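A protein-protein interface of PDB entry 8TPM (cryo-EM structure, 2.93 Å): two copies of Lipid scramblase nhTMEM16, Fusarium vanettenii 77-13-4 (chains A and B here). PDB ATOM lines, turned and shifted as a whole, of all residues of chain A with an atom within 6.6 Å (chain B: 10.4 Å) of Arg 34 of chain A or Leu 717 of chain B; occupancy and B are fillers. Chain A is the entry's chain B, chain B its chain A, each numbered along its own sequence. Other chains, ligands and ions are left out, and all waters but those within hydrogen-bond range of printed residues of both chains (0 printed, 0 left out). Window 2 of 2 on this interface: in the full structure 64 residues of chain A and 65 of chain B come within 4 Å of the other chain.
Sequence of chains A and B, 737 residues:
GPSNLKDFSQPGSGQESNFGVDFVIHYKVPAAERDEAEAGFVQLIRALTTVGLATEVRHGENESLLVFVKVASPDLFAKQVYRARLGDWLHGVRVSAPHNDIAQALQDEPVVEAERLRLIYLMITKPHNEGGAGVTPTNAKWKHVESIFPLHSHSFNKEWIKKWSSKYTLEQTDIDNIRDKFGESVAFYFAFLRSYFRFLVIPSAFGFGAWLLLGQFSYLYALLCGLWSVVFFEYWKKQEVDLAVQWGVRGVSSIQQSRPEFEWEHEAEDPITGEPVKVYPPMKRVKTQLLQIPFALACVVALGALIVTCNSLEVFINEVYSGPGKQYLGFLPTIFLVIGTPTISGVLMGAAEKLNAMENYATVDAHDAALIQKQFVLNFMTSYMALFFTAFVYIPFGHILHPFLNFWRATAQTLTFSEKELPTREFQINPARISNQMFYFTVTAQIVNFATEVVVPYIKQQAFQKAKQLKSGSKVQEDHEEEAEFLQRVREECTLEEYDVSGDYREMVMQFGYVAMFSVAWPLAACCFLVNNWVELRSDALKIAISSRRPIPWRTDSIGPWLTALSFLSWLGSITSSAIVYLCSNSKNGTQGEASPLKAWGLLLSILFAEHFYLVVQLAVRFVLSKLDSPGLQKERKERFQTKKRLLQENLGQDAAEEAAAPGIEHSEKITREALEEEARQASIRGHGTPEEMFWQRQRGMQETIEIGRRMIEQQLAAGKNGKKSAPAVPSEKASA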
ATOM      1  N   VAL A  29       6.854  30.724 -35.168  1.00  0.00           N
ATOM      2  CA  VAL A  29       7.321  29.784 -34.154  1.00  0.00           C
ATOM      3  C   VAL A  29       7.322  28.373 -34.732  1.00  0.00           C
ATOM      4  O   VAL A  29       6.248  27.785 -34.931  1.00  0.00           O
ATOM      5  CB  VAL A  29       6.459  29.858 -32.884  1.00  0.00           C
ATOM      6  CG1 VAL A  29       6.809  28.721 -31.933  1.00  0.00           C
ATOM      7  CG2 VAL A  29       6.636  31.202 -32.202  1.00  0.00           C
ATOM      8  N   PRO A  30       8.483  27.799 -35.026  1.00  0.00           N
ATOM      9  CA  PRO A  30       8.538  26.411 -35.488  1.00  0.00           C
ATOM     10  C   PRO A  30       8.693  25.431 -34.332  1.00  0.00           C
ATOM     11  O   PRO A  30       9.198  25.760 -33.257  1.00  0.00           O
ATOM     12  CB  PRO A  30       9.777  26.392 -36.398  1.00  0.00           C
ATOM     13  CG  PRO A  30      10.581  27.620 -36.023  1.00  0.00           C
ATOM     14  CD  PRO A  30       9.811  28.431 -35.019  1.00  0.00           C
ATOM     15  N   ALA A  31       8.240  24.201 -34.582  1.00  0.00           N
ATOM     16  CA  ALA A  31       8.240  23.181 -33.539  1.00  0.00           C
ATOM     17  C   ALA A  31       9.633  22.632 -33.260  1.00  0.00           C
ATOM     18  O   ALA A  31       9.874  22.100 -32.169  1.00  0.00           O
ATOM     19  CB  ALA A  31       7.297  22.039 -33.921  1.00  0.00           C
ATOM     20  N   ALA A  32      10.556  22.746 -34.217  1.00  0.00           N
ATOM     21  CA  ALA A  32      11.884  22.171 -34.038  1.00  0.00           C
ATOM     22  C   ALA A  32      12.738  22.956 -33.051  1.00  0.00           C
ATOM     23  O   ALA A  32      13.747  22.430 -32.571  1.00  0.00           O
ATOM     24  CB  ALA A  32      12.600  22.075 -35.387  1.00  0.00           C
ATOM     25  N   GLU A  33      12.363  24.193 -32.739  1.00  0.00           N
ATOM     26  CA  GLU A  33      13.101  25.047 -31.811  1.00  0.00           C
ATOM     27  C   GLU A  33      12.143  25.708 -30.827  1.00  0.00           C
ATOM     28  O   GLU A  33      12.167  26.921 -30.610  1.00  0.00           O
ATOM     29  CB  GLU A  33      13.922  26.089 -32.565  1.00  0.00           C
ATOM     30  CG  GLU A  33      13.191  26.763 -33.709  1.00  0.00           C
ATOM     31  CD  GLU A  33      13.650  26.264 -35.065  1.00  0.00           C
ATOM     32  OE1 GLU A  33      13.840  25.040 -35.216  1.00  0.00           O
ATOM     33  OE2 GLU A  33      13.824  27.097 -35.981  1.00  0.00           O
ATOM     34  N   ARG A  34      11.285  24.894 -30.210  1.00  0.00           N
ATOM     35  CA  ARG A  34      10.219  25.415 -29.358  1.00  0.00           C
ATOM     36  C   ARG A  34      10.765  26.132 -28.127  1.00  0.00           C
ATOM     37  O   ARG A  34      10.237  27.179 -27.730  1.00  0.00           O
ATOM     38  CB  ARG A  34       9.291  24.271 -28.947  1.00  0.00           C
ATOM     39  CG  ARG A  34       8.328  24.596 -27.818  1.00  0.00           C
ATOM     40  CD  ARG A  34       7.931  23.327 -27.081  1.00  0.00           C
ATOM     41  NE  ARG A  34       6.505  23.279 -26.776  1.00  0.00           N
ATOM     42  CZ  ARG A  34       5.999  23.319 -25.551  1.00  0.00           C
ATOM     43  NH1 ARG A  34       6.777  23.415 -24.484  1.00  0.00           N
ATOM     44  NH2 ARG A  34       4.681  23.257 -25.390  1.00  0.00           N
ATOM     45  N   ASP A  35      11.816  25.588 -27.510  1.00  0.00           N
ATOM     46  CA  ASP A  35      12.274  26.098 -26.219  1.00  0.00           C
ATOM     47  C   ASP A  35      12.784  27.532 -26.329  1.00  0.00           C
ATOM     48  O   ASP A  35      12.273  28.441 -25.661  1.00  0.00           O
ATOM     49  CB  ASP A  35      13.358  25.178 -25.653  1.00  0.00           C
ATOM     50  CG  ASP A  35      12.827  23.805 -25.292  1.00  0.00           C
ATOM     51  OD1 ASP A  35      11.877  23.341 -25.957  1.00  0.00           O
ATOM     52  OD2 ASP A  35      13.359  23.191 -24.343  1.00  0.00           O
ATOM     53  N   GLU A  36      13.803  27.754 -27.161  1.00  0.00           N
ATOM     54  CA  GLU A  36      14.344  29.101 -27.280  1.00  0.00           C
ATOM     55  C   GLU A  36      13.384  30.044 -27.994  1.00  0.00           C
ATOM     56  O   GLU A  36      13.461  31.254 -27.776  1.00  0.00           O
ATOM     57  CB  GLU A  36      15.703  29.082 -27.983  1.00  0.00           C
ATOM     58  CG  GLU A  36      15.658  29.215 -29.493  1.00  0.00           C
ATOM     59  CD  GLU A  36      15.622  27.873 -30.189  1.00  0.00           C
ATOM     60  OE1 GLU A  36      14.972  26.945 -29.665  1.00  0.00           O
ATOM     61  OE2 GLU A  36      16.256  27.745 -31.257  1.00  0.00           O
ATOM     62  N   ALA A  37      12.464  29.524 -28.810  1.00  0.00           N
ATOM     63  CA  ALA A  37      11.424  30.384 -29.367  1.00  0.00           C
ATOM     64  C   ALA A  37      10.508  30.917 -28.272  1.00  0.00           C
ATOM     65  O   ALA A  37      10.174  32.106 -28.258  1.00  0.00           O
ATOM     66  CB  ALA A  37      10.615  29.629 -30.421  1.00  0.00           C
ATOM     67  N   GLU A  38      10.097  30.051 -27.342  1.00  0.00           N
ATOM     68  CA  GLU A  38       9.299  30.500 -26.207  1.00  0.00           C
ATOM     69  C   GLU A  38      10.082  31.475 -25.334  1.00  0.00           C
ATOM     70  O   GLU A  38       9.530  32.473 -24.852  1.00  0.00           O
ATOM     71  CB  GLU A  38       8.839  29.293 -25.391  1.00  0.00           C
ATOM     72  CG  GLU A  38       8.127  29.637 -24.098  1.00  0.00           C
ATOM     73  CD  GLU A  38       8.840  29.074 -22.886  1.00  0.00           C
ATOM     74  OE1 GLU A  38       9.840  28.348 -23.069  1.00  0.00           O
ATOM     75  OE2 GLU A  38       8.406  29.357 -21.751  1.00  0.00           O
ATOM     76  N   ALA A  39      11.370  31.199 -25.119  1.00  0.00           N
ATOM     77  CA  ALA A  39      12.197  32.114 -24.337  1.00  0.00           C
ATOM     78  C   ALA A  39      12.287  33.484 -25.004  1.00  0.00           C
ATOM     79  O   ALA A  39      12.176  34.520 -24.336  1.00  0.00           O
ATOM     80  CB  ALA A  39      13.591  31.521 -24.135  1.00  0.00           C
ATOM     81  N   GLU A  63       2.094  28.159 -38.310  1.00  0.00           N
ATOM     82  CA  GLU A  63       3.043  28.017 -37.205  1.00  0.00           C
ATOM     83  C   GLU A  63       3.682  29.362 -36.852  1.00  0.00           C
ATOM     84  O   GLU A  63       4.893  29.561 -36.975  1.00  0.00           O
ATOM     85  CB  GLU A  63       4.112  26.963 -37.535  1.00  0.00           C
ATOM     86  CG  GLU A  63       3.733  25.469 -37.367  1.00  0.00           C
ATOM     87  CD  GLU A  63       2.843  25.111 -36.168  1.00  0.00           C
ATOM     88  OE1 GLU A  63       2.593  25.946 -35.275  1.00  0.00           O
ATOM     89  OE2 GLU A  63       2.378  23.952 -36.128  1.00  0.00           O
ATOM     90  N   GLY B 709       0.282  33.222 -23.491  1.00  0.00           N
ATOM     91  CA  GLY B 709       1.243  32.780 -24.488  1.00  0.00           C
ATOM     92  C   GLY B 709       1.645  31.327 -24.311  1.00  0.00           C
ATOM     93  O   GLY B 709       1.767  30.581 -25.289  1.00  0.00           O
ATOM     94  N   ARG B 710       1.864  30.906 -23.063  1.00  0.00           N
ATOM     95  CA  ARG B 710       2.192  29.508 -22.797  1.00  0.00           C
ATOM     96  C   ARG B 710       1.064  28.589 -23.253  1.00  0.00           C
ATOM     97  O   ARG B 710       1.301  27.569 -23.912  1.00  0.00           O
ATOM     98  CB  ARG B 710       2.478  29.297 -21.308  1.00  0.00           C
ATOM     99  CG  ARG B 710       3.598  30.148 -20.739  1.00  0.00           C
ATOM    100  CD  ARG B 710       4.936  29.861 -21.394  1.00  0.00           C
ATOM    101  NE  ARG B 710       5.963  30.785 -20.927  1.00  0.00           N
ATOM    102  CZ  ARG B 710       6.613  30.668 -19.778  1.00  0.00           C
ATOM    103  NH1 ARG B 710       6.371  29.669 -18.944  1.00  0.00           N
ATOM    104  NH2 ARG B 710       7.529  31.576 -19.455  1.00  0.00           N
ATOM    105  N   ARG B 711      -0.179  28.943 -22.912  1.00  0.00           N
ATOM    106  CA  ARG B 711      -1.314  28.134 -23.345  1.00  0.00           C
ATOM    107  C   ARG B 711      -1.449  28.123 -24.862  1.00  0.00           C
ATOM    108  O   ARG B 711      -1.824  27.097 -25.440  1.00  0.00           O
ATOM    109  CB  ARG B 711      -2.607  28.634 -22.700  1.00  0.00           C
ATOM    110  CG  ARG B 711      -2.570  28.679 -21.179  1.00  0.00           C
ATOM    111  CD  ARG B 711      -3.770  29.351 -20.454  1.00  0.00           C
ATOM    112  NE  ARG B 711      -4.371  30.537 -21.067  1.00  0.00           N
ATOM    113  CZ  ARG B 711      -5.116  30.557 -22.169  1.00  0.00           C
ATOM    114  NH1 ARG B 711      -5.522  29.442 -22.755  1.00  0.00           N
ATOM    115  NH2 ARG B 711      -5.501  31.728 -22.666  1.00  0.00           N
ATOM    116  N   MET B 712      -1.152  29.248 -25.518  1.00  0.00           N
ATOM    117  CA  MET B 712      -1.221  29.303 -26.975  1.00  0.00           C
ATOM    118  C   MET B 712      -0.194  28.373 -27.606  1.00  0.00           C
ATOM    119  O   MET B 712      -0.506  27.641 -28.552  1.00  0.00           O
ATOM    120  CB  MET B 712      -1.018  30.740 -27.455  1.00  0.00           C
ATOM    121  N   ILE B 713       1.042  28.391 -27.097  1.00  0.00           N
ATOM    122  CA  ILE B 713       2.050  27.440 -27.565  1.00  0.00           C
ATOM    123  C   ILE B 713       1.574  26.012 -27.341  1.00  0.00           C
ATOM    124  O   ILE B 713       1.732  25.142 -28.211  1.00  0.00           O
ATOM    125  CB  ILE B 713       3.409  27.697 -26.880  1.00  0.00           C
ATOM    126  CG1 ILE B 713       4.244  28.719 -27.655  1.00  0.00           C
ATOM    127  CG2 ILE B 713       4.195  26.404 -26.721  1.00  0.00           C
ATOM    128  CD1 ILE B 713       3.648  30.083 -27.739  1.00  0.00           C
ATOM    129  N   GLU B 714       0.974  25.749 -26.178  1.00  0.00           N
ATOM    130  CA  GLU B 714       0.512  24.400 -25.864  1.00  0.00           C
ATOM    131  C   GLU B 714      -0.523  23.923 -26.875  1.00  0.00           C
ATOM    132  O   GLU B 714      -0.407  22.822 -27.426  1.00  0.00           O
ATOM    133  CB  GLU B 714      -0.056  24.359 -24.447  1.00  0.00           C
ATOM    134  N   GLN B 715      -1.541  24.745 -27.146  1.00  0.00           N
ATOM    135  CA  GLN B 715      -2.591  24.304 -28.063  1.00  0.00           C
ATOM    136  C   GLN B 715      -2.103  24.289 -29.506  1.00  0.00           C
ATOM    137  O   GLN B 715      -2.619  23.516 -30.321  1.00  0.00           O
ATOM    138  CB  GLN B 715      -3.835  25.187 -27.950  1.00  0.00           C
ATOM    139  CG  GLN B 715      -3.569  26.670 -27.843  1.00  0.00           C
ATOM    140  CD  GLN B 715      -4.759  27.436 -27.297  1.00  0.00           C
ATOM    141  OE1 GLN B 715      -5.636  27.860 -28.048  1.00  0.00           O
ATOM    142  NE2 GLN B 715      -4.794  27.612 -25.981  1.00  0.00           N
ATOM    143  N   GLN B 716      -1.118  25.126 -29.843  1.00  0.00           N
ATOM    144  CA  GLN B 716      -0.626  25.161 -31.215  1.00  0.00           C
ATOM    145  C   GLN B 716       0.243  23.950 -31.525  1.00  0.00           C
ATOM    146  O   GLN B 716       0.150  23.376 -32.616  1.00  0.00           O
ATOM    147  CB  GLN B 716       0.146  26.458 -31.458  1.00  0.00           C
ATOM    148  CG  GLN B 716       0.664  26.615 -32.874  1.00  0.00           C
ATOM    149  CD  GLN B 716       0.919  28.063 -33.243  1.00  0.00           C
ATOM    150  OE1 GLN B 716       1.146  28.906 -32.376  1.00  0.00           O
ATOM    151  NE2 GLN B 716       0.881  28.360 -34.537  1.00  0.00           N
ATOM    152  N   LEU B 717       1.092  23.543 -30.581  1.00  0.00           N
ATOM    153  CA  LEU B 717       1.984  22.412 -30.796  1.00  0.00           C
ATOM    154  C   LEU B 717       1.451  21.109 -30.216  1.00  0.00           C
ATOM    155  O   LEU B 717       2.153  20.094 -30.263  1.00  0.00           O
ATOM    156  CB  LEU B 717       3.367  22.712 -30.210  1.00  0.00           C
ATOM    157  CG  LEU B 717       4.219  23.700 -31.012  1.00  0.00           C
ATOM    158  CD1 LEU B 717       5.689  23.540 -30.671  1.00  0.00           C
ATOM    159  CD2 LEU B 717       3.993  23.529 -32.508  1.00  0.00           C
ATOM    160  N   ALA B 718       0.232  21.107 -29.675  1.00  0.00           N
ATOM    161  CA  ALA B 718      -0.370  19.875 -29.180  1.00  0.00           C
ATOM    162  C   ALA B 718      -1.156  19.127 -30.248  1.00  0.00           C
ATOM    163  O   ALA B 718      -1.616  18.012 -29.987  1.00  0.00           O
ATOM    164  CB  ALA B 718      -1.285  20.179 -27.990  1.00  0.00           C
ATOM    165  N   ALA B 719      -1.321  19.706 -31.434  1.00  0.00           N
ATOM    166  CA  ALA B 719      -2.059  19.056 -32.509  1.00  0.00           C
ATOM    167  C   ALA B 719      -1.508  19.463 -33.872  1.00  0.00           C
ATOM    168  O   ALA B 719      -0.399  19.987 -33.971  1.00  0.00           O
ATOM    169  CB  ALA B 719      -3.539  19.389 -32.414  1.00  0.00           C
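Pro 30 of chain A touches none of the printed residues of chain B.
Ala 31 of chain A touches one residue of chain B.
Glu 33 of chain A touches none of the printed residues of chain B.
Of the printed residues of chain B, Arg 34 of chain A touches Ile 713 and Leu 717.
Glu 36 of chain A touches none of the printed residues of chain B.
Of the printed residues of chain B, Glu 38 of chain A touches Arg 710.
Of the printed residues of chain B, Glu 63 of chain A touches Gln 716 and Leu 717.
Of the printed residues of chain A, Leu 717 of chain B touches Ala 31 (3.9 Å), Arg 34 (3.99 Å) and Glu 63 (3.9 Å).
The nearest printed residue of chain B that does not touch Arg 34 of chain A is Glu 714 of chain B (4.3 Å).
The nearest printed residue of chain A that does not touch Leu 717 of chain B is Pro 30 of chain A (4.9 Å).
The nearest printed residue of chain B that does not touch Glu 63 of chain A is Ala 719 of chain B (5.3 Å).
The backbone NH of Val 29 of chain A is in hydrogen-bond range of the backbone carbonyl oxygen of Glu 63 of chain A.
Among the printed residues, pairs that only touch across the chains: Ala 31 of chain A with Leu 717 of chain B (3.9 Å), Arg 34 of chain A with Ile 713 of chain B (3.5 Å), Arg 34 of chain A with Leu 717 of chain B (3.99 Å) and Glu 63 of chain A with Leu 717 of chain B (3.9 Å).
OE1 of Glu 63 of chain A is in hydrogen-bond range of NE2 of Gln 716 of chain B (3.1 Å).
The guanidinium group (NE) of Arg 710 of chain B lies within salt-bridge range of the side-chain carboxylate (OE2) of Glu 38 of chain A (2.9 Å).
Of the 11 printed residues of chain B, 4 touch a printed residue of chain A.
Hydrophobic or aromatic side chains of chain B within 4 Å of the printed part of chain A: Ile 713 and Leu 717.
Hydrophobic or aromatic side chains of chain A within 4 Å of the printed part of chain B: Ala 31.
Among the printed residues, 6 pairs touch across the chains.
Among the printed residues, Asp or Glu carboxylates within 4 Å of a Lys or Arg side-chain nitrogen of the other chain: Glu 38 of chain A with Arg 710 of chain B (2.9 Å).
No position is printed for both chains.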
